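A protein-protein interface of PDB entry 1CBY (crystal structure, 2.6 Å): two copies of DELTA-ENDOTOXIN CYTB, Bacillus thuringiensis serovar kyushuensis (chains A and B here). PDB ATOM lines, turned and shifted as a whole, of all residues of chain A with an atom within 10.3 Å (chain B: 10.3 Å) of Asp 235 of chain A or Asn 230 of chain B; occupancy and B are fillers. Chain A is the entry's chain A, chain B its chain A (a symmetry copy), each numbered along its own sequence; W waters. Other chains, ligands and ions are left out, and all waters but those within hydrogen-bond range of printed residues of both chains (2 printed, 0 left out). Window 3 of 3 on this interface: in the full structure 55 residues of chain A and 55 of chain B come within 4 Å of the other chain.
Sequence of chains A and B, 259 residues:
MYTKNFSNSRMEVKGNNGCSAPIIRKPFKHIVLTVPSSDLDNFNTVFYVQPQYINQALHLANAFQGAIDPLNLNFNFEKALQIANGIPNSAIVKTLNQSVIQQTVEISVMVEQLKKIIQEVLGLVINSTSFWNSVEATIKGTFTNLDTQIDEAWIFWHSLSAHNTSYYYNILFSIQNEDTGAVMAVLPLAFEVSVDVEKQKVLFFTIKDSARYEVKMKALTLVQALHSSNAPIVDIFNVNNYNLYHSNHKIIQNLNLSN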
ATOM      1  N   SER A  38       7.470  -0.474 -26.185  1.00  0.00           N
ATOM      2  CA  SER A  38       7.391  -0.867 -27.588  1.00  0.00           C
ATOM      3  C   SER A  38       6.358  -1.974 -27.781  1.00  0.00           C
ATOM      4  O   SER A  38       5.924  -2.241 -28.901  1.00  0.00           O
ATOM      5  CB  SER A  38       8.757  -1.349 -28.090  1.00  0.00           C
ATOM      6  OG  SER A  38       9.660  -0.266 -28.260  1.00  0.00           O
ATOM      7  N   ILE A  54      20.559  -4.872 -16.626  1.00  0.00           N
ATOM      8  CA  ILE A  54      19.216  -4.346 -16.832  1.00  0.00           C
ATOM      9  C   ILE A  54      18.618  -4.945 -18.101  1.00  0.00           C
ATOM     10  O   ILE A  54      17.454  -5.345 -18.117  1.00  0.00           O
ATOM     11  CB  ILE A  54      19.224  -2.792 -16.900  1.00  0.00           C
ATOM     12  CG1 ILE A  54      19.461  -2.215 -15.496  1.00  0.00           C
ATOM     13  CG2 ILE A  54      17.926  -2.265 -17.511  1.00  0.00           C
ATOM     14  CD1 ILE A  54      19.656  -0.715 -15.451  1.00  0.00           C
ATOM     15  N   ASN A  55      19.437  -5.064 -19.143  1.00  0.00           N
ATOM     16  CA  ASN A  55      18.996  -5.624 -20.418  1.00  0.00           C
ATOM     17  C   ASN A  55      18.487  -7.046 -20.211  1.00  0.00           C
ATOM     18  O   ASN A  55      17.423  -7.409 -20.706  1.00  0.00           O
ATOM     19  CB  ASN A  55      20.151  -5.629 -21.421  1.00  0.00           C
ATOM     20  CG  ASN A  55      19.681  -5.665 -22.872  1.00  0.00           C
ATOM     21  OD1 ASN A  55      20.464  -5.390 -23.782  1.00  0.00           O
ATOM     22  ND2 ASN A  55      18.411  -5.988 -23.096  1.00  0.00           N
ATOM     23  N   LEU A  58      15.173  -6.993 -18.358  1.00  0.00           N
ATOM     24  CA  LEU A  58      14.121  -6.517 -19.241  1.00  0.00           C
ATOM     25  C   LEU A  58      13.685  -7.625 -20.198  1.00  0.00           C
ATOM     26  O   LEU A  58      12.493  -7.778 -20.485  1.00  0.00           O
ATOM     27  CB  LEU A  58      14.610  -5.284 -20.001  1.00  0.00           C
ATOM     28  CG  LEU A  58      13.599  -4.167 -20.271  1.00  0.00           C
ATOM     29  CD1 LEU A  58      12.689  -3.941 -19.069  1.00  0.00           C
ATOM     30  CD2 LEU A  58      14.348  -2.896 -20.617  1.00  0.00           C
ATOM     31  N   HIS A  59      14.642  -8.415 -20.668  1.00  0.00           N
ATOM     32  CA  HIS A  59      14.336  -9.519 -21.563  1.00  0.00           C
ATOM     33  C   HIS A  59      13.454 -10.529 -20.844  1.00  0.00           C
ATOM     34  O   HIS A  59      12.394 -10.909 -21.345  1.00  0.00           O
ATOM     35  CB  HIS A  59      15.614 -10.199 -22.039  1.00  0.00           C
ATOM     36  CG  HIS A  59      16.206  -9.573 -23.261  1.00  0.00           C
ATOM     37  ND1 HIS A  59      16.509  -8.236 -23.312  1.00  0.00           N
ATOM     38  CD2 HIS A  59      16.496 -10.146 -24.457  1.00  0.00           C
ATOM     39  CE1 HIS A  59      16.971  -8.022 -24.529  1.00  0.00           C
ATOM     40  NE2 HIS A  59      16.982  -9.147 -25.260  1.00  0.00           N
ATOM     41  N   ASN A  62       9.868  -9.157 -20.285  1.00  0.00           N
ATOM     42  CA  ASN A  62       9.071  -9.211 -21.510  1.00  0.00           C
ATOM     43  C   ASN A  62       8.642 -10.616 -21.877  1.00  0.00           C
ATOM     44  O   ASN A  62       7.521 -10.818 -22.345  1.00  0.00           O
ATOM     45  CB  ASN A  62       9.826  -8.604 -22.690  1.00  0.00           C
ATOM     46  CG  ASN A  62       9.987  -7.108 -22.572  1.00  0.00           C
ATOM     47  OD1 ASN A  62       9.416  -6.472 -21.677  1.00  0.00           O
ATOM     48  ND2 ASN A  62      10.769  -6.530 -23.473  1.00  0.00           N
ATOM     49  N   SER A 229      25.581  -6.732 -20.354  1.00  0.00           N
ATOM     50  CA  SER A 229      25.301  -6.013 -21.593  1.00  0.00           C
ATOM     51  C   SER A 229      25.381  -4.501 -21.417  1.00  0.00           C
ATOM     52  O   SER A 229      24.713  -3.930 -20.553  1.00  0.00           O
ATOM     53  CB  SER A 229      23.919  -6.376 -22.132  1.00  0.00           C
ATOM     54  OG  SER A 229      23.579  -5.546 -23.235  1.00  0.00           O
ATOM     55  N   ASN A 230      26.180  -3.856 -22.264  1.00  0.00           N
ATOM     56  CA  ASN A 230      26.346  -2.405 -22.229  1.00  0.00           C
ATOM     57  C   ASN A 230      25.858  -1.825 -23.560  1.00  0.00           C
ATOM     58  O   ASN A 230      26.516  -0.985 -24.176  1.00  0.00           O
ATOM     59  CB  ASN A 230      27.816  -2.041 -21.988  1.00  0.00           C
ATOM     60  CG  ASN A 230      28.028  -0.549 -21.792  1.00  0.00           C
ATOM     61  OD1 ASN A 230      27.114   0.177 -21.394  1.00  0.00           O
ATOM     62  ND2 ASN A 230      29.236  -0.084 -22.067  1.00  0.00           N
ATOM     63  N   ALA A 231      24.699  -2.313 -23.999  1.00  0.00           N
ATOM     64  CA  ALA A 231      24.074  -1.896 -25.252  1.00  0.00           C
ATOM     65  C   ALA A 231      23.527  -0.480 -25.160  1.00  0.00           C
ATOM     66  O   ALA A 231      23.386   0.061 -24.066  1.00  0.00           O
ATOM     67  CB  ALA A 231      22.951  -2.859 -25.601  1.00  0.00           C
ATOM     68  N   PRO A 232      23.270   0.164 -26.312  1.00  0.00           N
ATOM     69  CA  PRO A 232      22.732   1.529 -26.325  1.00  0.00           C
ATOM     70  C   PRO A 232      21.374   1.518 -25.622  1.00  0.00           C
ATOM     71  O   PRO A 232      20.480   0.750 -25.996  1.00  0.00           O
ATOM     72  CB  PRO A 232      22.595   1.816 -27.817  1.00  0.00           C
ATOM     73  CG  PRO A 232      23.722   1.059 -28.398  1.00  0.00           C
ATOM     74  CD  PRO A 232      23.612  -0.261 -27.679  1.00  0.00           C
ATOM     75  N   ILE A 233      21.229   2.365 -24.607  1.00  0.00           N
ATOM     76  CA  ILE A 233      20.005   2.428 -23.815  1.00  0.00           C
ATOM     77  C   ILE A 233      18.697   2.386 -24.607  1.00  0.00           C
ATOM     78  O   ILE A 233      17.768   1.666 -24.231  1.00  0.00           O
ATOM     79  CB  ILE A 233      20.031   3.621 -22.832  1.00  0.00           C
ATOM     80  CG1 ILE A 233      18.866   3.514 -21.850  1.00  0.00           C
ATOM     81  CG2 ILE A 233      20.011   4.944 -23.584  1.00  0.00           C
ATOM     82  CD1 ILE A 233      18.882   4.577 -20.779  1.00  0.00           C
ATOM     83  N   VAL A 234      18.632   3.100 -25.727  1.00  0.00           N
ATOM     84  CA  VAL A 234      17.412   3.101 -26.533  1.00  0.00           C
ATOM     85  C   VAL A 234      17.187   1.723 -27.146  1.00  0.00           C
ATOM     86  O   VAL A 234      16.064   1.217 -27.158  1.00  0.00           O
ATOM     87  CB  VAL A 234      17.450   4.164 -27.656  1.00  0.00           C
ATOM     88  CG1 VAL A 234      16.152   4.132 -28.445  1.00  0.00           C
ATOM     89  CG2 VAL A 234      17.678   5.554 -27.067  1.00  0.00           C
ATOM     90  N   ASP A 235      18.262   1.103 -27.617  1.00  0.00           N
ATOM     91  CA  ASP A 235      18.169  -0.219 -28.222  1.00  0.00           C
ATOM     92  C   ASP A 235      17.530  -1.167 -27.224  1.00  0.00           C
ATOM     93  O   ASP A 235      16.695  -1.995 -27.585  1.00  0.00           O
ATOM     94  CB  ASP A 235      19.559  -0.750 -28.596  1.00  0.00           C
ATOM     95  CG  ASP A 235      20.199   0.009 -29.751  1.00  0.00           C
ATOM     96  OD1 ASP A 235      19.747   1.130 -30.082  1.00  0.00           O
ATOM     97  OD2 ASP A 235      21.175  -0.521 -30.329  1.00  0.00           O
ATOM     98  N   ILE A 236      17.904  -1.013 -25.959  1.00  0.00           N
ATOM     99  CA  ILE A 236      17.371  -1.862 -24.902  1.00  0.00           C
ATOM    100  C   ILE A 236      15.849  -1.756 -24.805  1.00  0.00           C
ATOM    101  O   ILE A 236      15.152  -2.767 -24.828  1.00  0.00           O
ATOM    102  CB  ILE A 236      18.034  -1.541 -23.528  1.00  0.00           C
ATOM    103  CG1 ILE A 236      19.524  -1.896 -23.576  1.00  0.00           C
ATOM    104  CG2 ILE A 236      17.351  -2.311 -22.404  1.00  0.00           C
ATOM    105  CD1 ILE A 236      20.268  -1.632 -22.293  1.00  0.00           C
ATOM    106  N   PHE A 237      15.329  -0.536 -24.768  1.00  0.00           N
ATOM    107  CA  PHE A 237      13.888  -0.346 -24.662  1.00  0.00           C
ATOM    108  C   PHE A 237      13.094  -0.573 -25.949  1.00  0.00           C
ATOM    109  O   PHE A 237      11.869  -0.474 -25.946  1.00  0.00           O
ATOM    110  CB  PHE A 237      13.577   1.015 -24.041  1.00  0.00           C
ATOM    111  CG  PHE A 237      13.986   1.118 -22.596  1.00  0.00           C
ATOM    112  CD1 PHE A 237      15.270   1.522 -22.247  1.00  0.00           C
ATOM    113  CD2 PHE A 237      13.098   0.770 -21.583  1.00  0.00           C
ATOM    114  CE1 PHE A 237      15.665   1.574 -20.909  1.00  0.00           C
ATOM    115  CE2 PHE A 237      13.487   0.819 -20.243  1.00  0.00           C
ATOM    116  CZ  PHE A 237      14.771   1.221 -19.908  1.00  0.00           C
ATOM    117  N   ASN A 238      13.780  -0.881 -27.044  1.00  0.00           N
ATOM    118  CA  ASN A 238      13.109  -1.150 -28.318  1.00  0.00           C
ATOM    119  C   ASN A 238      12.731  -2.621 -28.430  1.00  0.00           C
ATOM    120  O   ASN A 238      11.972  -3.008 -29.321  1.00  0.00           O
ATOM    121  CB  ASN A 238      14.002  -0.782 -29.505  1.00  0.00           C
ATOM    122  CG  ASN A 238      13.909   0.684 -29.891  1.00  0.00           C
ATOM    123  OD1 ASN A 238      14.563   1.120 -30.838  1.00  0.00           O
ATOM    124  ND2 ASN A 238      13.098   1.452 -29.171  1.00  0.00           N
ATOM    125  N   VAL A 239      13.295  -3.444 -27.553  1.00  0.00           N
ATOM    126  CA  VAL A 239      13.021  -4.877 -27.558  1.00  0.00           C
ATOM    127  C   VAL A 239      11.534  -5.118 -27.297  1.00  0.00           C
ATOM    128  O   VAL A 239      10.936  -4.482 -26.431  1.00  0.00           O
ATOM    129  CB  VAL A 239      13.881  -5.615 -26.491  1.00  0.00           C
ATOM    130  CG1 VAL A 239      13.558  -7.103 -26.473  1.00  0.00           C
ATOM    131  CG2 VAL A 239      15.369  -5.403 -26.768  1.00  0.00           C
ATOM    132  N   ASN A 240      10.937  -6.022 -28.063  1.00  0.00           N
ATOM    133  CA  ASN A 240       9.519  -6.327 -27.903  1.00  0.00           C
ATOM    134  C   ASN A 240       9.331  -7.634 -27.157  1.00  0.00           C
ATOM    135  O   ASN A 240      10.297  -8.205 -26.661  1.00  0.00           O
ATOM    136  CB  ASN A 240       8.812  -6.368 -29.264  1.00  0.00           C
ATOM    137  CG  ASN A 240       9.426  -7.370 -30.238  1.00  0.00           C
ATOM    138  OD1 ASN A 240       9.103  -7.350 -31.419  1.00  0.00           O
ATOM    139  ND2 ASN A 240      10.306  -8.239 -29.755  1.00  0.00           N
ATOM    140  N   LEU A 244      12.175 -14.503 -27.710  1.00  0.00           N
ATOM    141  CA  LEU A 244      12.925 -14.417 -26.462  1.00  0.00           C
ATOM    142  C   LEU A 244      13.223 -15.758 -25.789  1.00  0.00           C
ATOM    143  O   LEU A 244      14.141 -15.848 -24.968  1.00  0.00           O
ATOM    144  CB  LEU A 244      12.219 -13.471 -25.482  1.00  0.00           C
ATOM    145  CG  LEU A 244      12.112 -11.997 -25.883  1.00  0.00           C
ATOM    146  CD1 LEU A 244      11.450 -11.201 -24.783  1.00  0.00           C
ATOM    147  CD2 LEU A 244      13.485 -11.427 -26.185  1.00  0.00           C
ATOM    148  N   LYS B  29       5.892   1.193 -19.501  1.00  0.00           N
ATOM    149  CA  LYS B  29       6.540   0.307 -18.551  1.00  0.00           C
ATOM    150  C   LYS B  29       6.586   1.051 -17.225  1.00  0.00           C
ATOM    151  O   LYS B  29       6.790   2.266 -17.197  1.00  0.00           O
ATOM    152  CB  LYS B  29       7.957  -0.046 -19.004  1.00  0.00           C
ATOM    153  CG  LYS B  29       8.000  -0.981 -20.192  1.00  0.00           C
ATOM    154  CD  LYS B  29       9.407  -1.471 -20.457  1.00  0.00           C
ATOM    155  CE  LYS B  29       9.409  -2.595 -21.483  1.00  0.00           C
ATOM    156  NZ  LYS B  29       8.551  -3.734 -21.044  1.00  0.00           N
ATOM    157  N   GLN B  50      11.255   9.576 -22.070  1.00  0.00           N
ATOM    158  CA  GLN B  50      11.512   8.589 -23.114  1.00  0.00           C
ATOM    159  C   GLN B  50      12.948   8.081 -22.946  1.00  0.00           C
ATOM    160  O   GLN B  50      13.820   8.809 -22.470  1.00  0.00           O
ATOM    161  CB  GLN B  50      11.305   9.216 -24.492  1.00  0.00           C
ATOM    162  CG  GLN B  50       9.847   9.544 -24.781  1.00  0.00           C
ATOM    163  CD  GLN B  50       9.659  10.282 -26.088  1.00  0.00           C
ATOM    164  OE1 GLN B  50       9.025  11.334 -26.130  1.00  0.00           O
ATOM    165  NE2 GLN B  50      10.207   9.738 -27.163  1.00  0.00           N
ATOM    166  N   PRO B  51      13.222   6.833 -23.364  1.00  0.00           N
ATOM    167  CA  PRO B  51      14.557   6.241 -23.244  1.00  0.00           C
ATOM    168  C   PRO B  51      15.719   7.142 -23.650  1.00  0.00           C
ATOM    169  O   PRO B  51      16.665   7.317 -22.885  1.00  0.00           O
ATOM    170  CB  PRO B  51      14.460   5.013 -24.145  1.00  0.00           C
ATOM    171  CG  PRO B  51      13.023   4.604 -23.988  1.00  0.00           C
ATOM    172  CD  PRO B  51      12.320   5.935 -24.108  1.00  0.00           C
ATOM    173  N   GLN B  52      15.639   7.739 -24.834  1.00  0.00           N
ATOM    174  CA  GLN B  52      16.715   8.598 -25.311  1.00  0.00           C
ATOM    175  C   GLN B  52      16.956   9.863 -24.490  1.00  0.00           C
ATOM    176  O   GLN B  52      17.925  10.584 -24.736  1.00  0.00           O
ATOM    177  CB  GLN B  52      16.522   8.964 -26.786  1.00  0.00           C
ATOM    178  CG  GLN B  52      15.250   9.723 -27.100  1.00  0.00           C
ATOM    179  CD  GLN B  52      14.108   8.802 -27.456  1.00  0.00           C
ATOM    180  OE1 GLN B  52      13.446   8.242 -26.582  1.00  0.00           O
ATOM    181  NE2 GLN B  52      13.876   8.629 -28.748  1.00  0.00           N
ATOM    182  N   TYR B  53      16.092  10.132 -23.518  1.00  0.00           N
ATOM    183  CA  TYR B  53      16.236  11.319 -22.680  1.00  0.00           C
ATOM    184  C   TYR B  53      16.512  10.967 -21.220  1.00  0.00           C
ATOM    185  O   TYR B  53      16.573  11.846 -20.354  1.00  0.00           O
ATOM    186  CB  TYR B  53      14.989  12.203 -22.791  1.00  0.00           C
ATOM    187  CG  TYR B  53      14.737  12.715 -24.190  1.00  0.00           C
ATOM    188  CD1 TYR B  53      15.622  13.607 -24.792  1.00  0.00           C
ATOM    189  CD2 TYR B  53      13.628  12.291 -24.918  1.00  0.00           C
ATOM    190  CE1 TYR B  53      15.415  14.060 -26.086  1.00  0.00           C
ATOM    191  CE2 TYR B  53      13.409  12.740 -26.215  1.00  0.00           C
ATOM    192  CZ  TYR B  53      14.305  13.626 -26.795  1.00  0.00           C
ATOM    193  OH  TYR B  53      14.093  14.082 -28.078  1.00  0.00           O
ATOM    194  N   ILE B  54      16.704   9.680 -20.954  1.00  0.00           N
ATOM    195  CA  ILE B  54      16.983   9.213 -19.603  1.00  0.00           C
ATOM    196  C   ILE B  54      18.323   9.772 -19.132  1.00  0.00           C
ATOM    197  O   ILE B  54      18.446  10.228 -17.996  1.00  0.00           O
ATOM    198  CB  ILE B  54      16.970   7.659 -19.530  1.00  0.00           C
ATOM    199  CG1 ILE B  54      15.526   7.149 -19.634  1.00  0.00           C
ATOM    200  CG2 ILE B  54      17.649   7.166 -18.252  1.00  0.00           C
ATOM    201  CD1 ILE B  54      15.389   5.645 -19.742  1.00  0.00           C
ATOM    202  N   ASN B  55      19.305   9.790 -20.029  1.00  0.00           N
ATOM    203  CA  ASN B  55      20.636  10.301 -19.712  1.00  0.00           C
ATOM    204  C   ASN B  55      20.541  11.757 -19.269  1.00  0.00           C
ATOM    205  O   ASN B  55      21.131  12.145 -18.265  1.00  0.00           O
ATOM    206  CB  ASN B  55      21.548  10.193 -20.935  1.00  0.00           C
ATOM    207  CG  ASN B  55      23.031  10.172 -20.574  1.00  0.00           C
ATOM    208  OD1 ASN B  55      23.864   9.808 -21.404  1.00  0.00           O
ATOM    209  ND2 ASN B  55      23.366  10.546 -19.343  1.00  0.00           N
ATOM    210  N   GLN B  56      19.778  12.554 -20.011  1.00  0.00           N
ATOM    211  CA  GLN B  56      19.594  13.966 -19.691  1.00  0.00           C
ATOM    212  C   GLN B  56      18.944  14.125 -18.323  1.00  0.00           C
ATOM    213  O   GLN B  56      19.364  14.955 -17.515  1.00  0.00           O
ATOM    214  CB  GLN B  56      18.729  14.641 -20.757  1.00  0.00           C
ATOM    215  CG  GLN B  56      18.453  16.115 -20.507  1.00  0.00           C
ATOM    216  CD  GLN B  56      17.651  16.756 -21.623  1.00  0.00           C
ATOM    217  OE1 GLN B  56      17.222  16.084 -22.564  1.00  0.00           O
ATOM    218  NE2 GLN B  56      17.446  18.061 -21.527  1.00  0.00           N
ATOM    219  N   HIS B 227      17.741  16.964 -25.130  1.00  0.00           N
ATOM    220  CA  HIS B 227      19.026  16.475 -25.610  1.00  0.00           C
ATOM    221  C   HIS B 227      19.010  14.949 -25.655  1.00  0.00           C
ATOM    222  O   HIS B 227      19.121  14.281 -24.625  1.00  0.00           O
ATOM    223  CB  HIS B 227      20.147  16.974 -24.697  1.00  0.00           C
ATOM    224  CG  HIS B 227      21.511  16.791 -25.272  1.00  0.00           C
ATOM    225  ND1 HIS B 227      22.009  17.653 -26.219  1.00  0.00           N
ATOM    226  CD2 HIS B 227      22.398  15.785 -25.070  1.00  0.00           C
ATOM    227  CE1 HIS B 227      23.177  17.156 -26.575  1.00  0.00           C
ATOM    228  NE2 HIS B 227      23.457  16.025 -25.907  1.00  0.00           N
ATOM    229  N   SER B 228      18.858  14.405 -26.857  1.00  0.00           N
ATOM    230  CA  SER B 228      18.798  12.963 -27.060  1.00  0.00           C
ATOM    231  C   SER B 228      20.150  12.287 -26.872  1.00  0.00           C
ATOM    232  O   SER B 228      21.179  12.852 -27.233  1.00  0.00           O
ATOM    233  CB  SER B 228      18.251  12.667 -28.458  1.00  0.00           C
ATOM    234  OG  SER B 228      18.125  11.275 -28.689  1.00  0.00           O
ATOM    235  N   SER B 229      20.137  11.073 -26.327  1.00  0.00           N
ATOM    236  CA  SER B 229      21.354  10.302 -26.097  1.00  0.00           C
ATOM    237  C   SER B 229      21.096   8.800 -26.081  1.00  0.00           C
ATOM    238  O   SER B 229      20.256   8.312 -25.323  1.00  0.00           O
ATOM    239  CB  SER B 229      22.013  10.705 -24.780  1.00  0.00           C
ATOM    240  OG  SER B 229      23.094   9.834 -24.475  1.00  0.00           O
ATOM    241  N   ASN B 230      21.845   8.070 -26.902  1.00  0.00           N
ATOM    242  CA  ASN B 230      21.724   6.615 -26.985  1.00  0.00           C
ATOM    243  C   ASN B 230      23.057   5.989 -26.563  1.00  0.00           C
ATOM    244  O   ASN B 230      23.578   5.084 -27.216  1.00  0.00           O
ATOM    245  CB  ASN B 230      21.356   6.191 -28.412  1.00  0.00           C
ATOM    246  CG  ASN B 230      21.068   4.703 -28.526  1.00  0.00           C
ATOM    247  OD1 ASN B 230      20.704   4.049 -27.548  1.00  0.00           O
ATOM    248  ND2 ASN B 230      21.228   4.163 -29.724  1.00  0.00           N
ATOM    249  N   ALA B 231      23.606   6.510 -25.468  1.00  0.00           N
ATOM    250  CA  ALA B 231      24.880   6.058 -24.912  1.00  0.00           C
ATOM    251  C   ALA B 231      24.757   4.679 -24.283  1.00  0.00           C
ATOM    252  O   ALA B 231      23.649   4.207 -24.034  1.00  0.00           O
ATOM    253  CB  ALA B 231      25.361   7.056 -23.873  1.00  0.00           C
ATOM    254  N   PRO B 232      25.889   3.987 -24.075  1.00  0.00           N
ATOM    255  CA  PRO B 232      25.873   2.651 -23.465  1.00  0.00           C
ATOM    256  C   PRO B 232      25.276   2.771 -22.063  1.00  0.00           C
ATOM    257  O   PRO B 232      25.754   3.562 -21.241  1.00  0.00           O
ATOM    258  CB  PRO B 232      27.355   2.291 -23.420  1.00  0.00           C
ATOM    259  CG  PRO B 232      27.887   2.956 -24.626  1.00  0.00           C
ATOM    260  CD  PRO B 232      27.246   4.318 -24.537  1.00  0.00           C
ATOM    261  N   ILE B 233      24.232   1.990 -21.798  1.00  0.00           N
ATOM    262  CA  ILE B 233      23.531   2.034 -20.518  1.00  0.00           C
ATOM    263  C   ILE B 233      24.421   2.098 -19.275  1.00  0.00           C
ATOM    264  O   ILE B 233      24.152   2.885 -18.363  1.00  0.00           O
ATOM    265  CB  ILE B 233      22.490   0.897 -20.408  1.00  0.00           C
ATOM    266  CG1 ILE B 233      21.605   1.117 -19.183  1.00  0.00           C
ATOM    267  CG2 ILE B 233      23.173  -0.463 -20.370  1.00  0.00           C
ATOM    268  CD1 ILE B 233      20.482   0.114 -19.063  1.00  0.00           C
ATOM    269  N   VAL B 234      25.504   1.329 -19.252  1.00  0.00           N
ATOM    270  CA  VAL B 234      26.398   1.345 -18.095  1.00  0.00           C
ATOM    271  C   VAL B 234      27.096   2.698 -17.991  1.00  0.00           C
ATOM    272  O   VAL B 234      27.218   3.258 -16.901  1.00  0.00           O
ATOM    273  CB  VAL B 234      27.460   0.222 -18.155  1.00  0.00           C
ATOM    274  CG1 VAL B 234      28.344   0.277 -16.921  1.00  0.00           C
ATOM    275  CG2 VAL B 234      26.785  -1.143 -18.264  1.00  0.00           C
ATOM    276  N   ASP B 235      27.517   3.234 -19.129  1.00  0.00           N
ATOM    277  CA  ASP B 235      28.193   4.525 -19.153  1.00  0.00           C
ATOM    278  C   ASP B 235      27.295   5.556 -18.497  1.00  0.00           C
ATOM    279  O   ASP B 235      27.760   6.406 -17.738  1.00  0.00           O
ATOM    280  CB  ASP B 235      28.489   4.962 -20.594  1.00  0.00           C
ATOM    281  CG  ASP B 235      29.552   4.109 -21.273  1.00  0.00           C
ATOM    282  OD1 ASP B 235      29.859   2.996 -20.784  1.00  0.00           O
ATOM    283  OD2 ASP B 235      30.082   4.556 -22.315  1.00  0.00           O
ATOM    284  N   ILE B 236      26.000   5.454 -18.769  1.00  0.00           N
ATOM    285  CA  ILE B 236      25.031   6.386 -18.210  1.00  0.00           C
ATOM    286  C   ILE B 236      25.043   6.363 -16.681  1.00  0.00           C
ATOM    287  O   ILE B 236      25.169   7.406 -16.045  1.00  0.00           O
ATOM    288  CB  ILE B 236      23.597   6.107 -18.753  1.00  0.00           C
ATOM    289  CG1 ILE B 236      23.550   6.383 -20.261  1.00  0.00           C
ATOM    290  CG2 ILE B 236      22.567   6.972 -18.034  1.00  0.00           C
ATOM    291  CD1 ILE B 236      22.204   6.152 -20.894  1.00  0.00           C
HETATM  292  O   HOH W   1       8.296  -5.930 -19.213  1.00  0.00           O
HETATM  293  O   HOH W   2       7.081  -4.787 -23.389  1.00  0.00           O
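The backbone carbonyl oxygen (O) of Gln 52 of chain B sits at hydrogen-bond distance from the backbone NH (N) of Ser 229 of chain B (2.8 Å). The side-chain amide oxygen (OD1) of Asn 55 of chain B sits at hydrogen-bond distance from the side-chain hydroxyl (OG) of Ser 229 of chain B, at 3.2 Å.
Ser 229 of chain A touches Ile 233 of chain B, and with the chains exchanged Ile 233 of chain A touches Ser 229 of chain B. Ala 231 of chain A touches Pro 232 of chain B, and with the chains exchanged Pro 232 of chain A touches Ala 231 of chain B. Of the 21 pairs that touch across the chains among the printed residues, 18 have their exchanged pair printed and touching as well.
The side-chain amino group (NZ) of Lys 29 of chain B sits at hydrogen-bond distance from the side-chain amide oxygen (OD1) of Asn 62 of chain A (2.9 Å). OD1 of Asn 230 of chain A is in hydrogen-bond range of N of Ile 233 of chain B, 3.4 Å away. The side-chain amide oxygen of Asn 230 of chain A is in hydrogen-bond range of the backbone NH of Val 234 of chain B, 2.9 Å away. The side-chain amide nitrogen (ND2) of Asn 230 of chain A sits at hydrogen-bond distance from the side-chain carboxylate (OD1) of Asp 235 of chain B (3.4 Å). The backbone carbonyl oxygen (O) of Ala 231 of chain A is in hydrogen-bond range of the backbone NH (N) of Ile 233 of chain B, 3.1 Å away. N of Ile 233 of chain A sits at hydrogen-bond distance from OD1 of Asn 230 of chain B (3.4 Å). N of Ile 233 of chain A is in hydrogen-bond range of O of Ala 231 of chain B, 3.1 Å away. The side-chain amide oxygen (OD1) of Asn 230 of chain B sits at hydrogen-bond distance from the backbone NH (N) of Val 234 of chain A, at 2.9 Å. ND2 of Asn 230 of chain B is in hydrogen-bond range of OD1 of Asp 235 of chain A, at 3.4 Å.
Hydrophobic or aromatic side chains of chain B that line the printed part of chain A: Pro 51, Ile 54, Pro 232, Ile 233, Val 234 and Ile 236.
Among the printed residues, merely in contact across the chains: Ile 54 of chain A with Ile 233 of chain B, Ser 229 of chain A with Ile 233 of chain B, Asn 230 of chain A with Pro 232 of chain B, Ala 231 of chain A with Pro 232 of chain B, Pro 232 of chain A with Asn 230 of chain B, Pro 232 of chain A with Ala 231 of chain B, Ile 233 of chain A with Ile 54 of chain B, Ile 233 of chain A with Ser 229 of chain B, Ile 233 of chain A with Ile 236 of chain B, Val 234 of chain A with Gln 52 of chain B, Ile 236 of chain A with Ile 233 of chain B and Phe 237 of chain A with Pro 51 of chain B.
Water W1 bridges the side-chain amide oxygen of Asn 62 of chain A and the side-chain amino group of Lys 29 of chain B. Water W2 bridges the side-chain amino group (NZ) of Lys 29 of chain B (3.0 Å) and the side-chain amide oxygen (OD1) of Asn 62 of chain A (3.3 Å).
Of chain A, only Pro 232 (2.9 Å), Ile 233 (3.4 Å), Val 234 (2.9 Å) and Asp 235 (3.4 Å) come within 4 Å of Asn 230 of chain B. Of the printed residues of chain B, Pro 232 of chain A touches Asn 230 and Ala 231. Val 234 of chain A touches just these residues of chain B: Gln 52 (3.6 Å) and Asn 230 (2.9 Å). Ile 236 of chain A touches just one residue of chain B: Ile 233. No residue of chain B comes within 4 Å of Asn 238 of chain A. Ser 229 of chain B touches just one residue of chain A: Ile 233. Of the printed residues of chain B, Asn 62 of chain A touches Lys 29. Of the printed residues of chain B, Asn 230 of chain A touches Pro 232 (2.9 Å), Ile 233 (3.4 Å), Val 234 (2.9 Å) and Asp 235 (3.4 Å). Asn 240 of chain A touches none of the printed residues of chain B. The nearest printed residue of chain B that does not touch Asn 62 of chain A is Pro 51 of chain B (11.4 Å).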
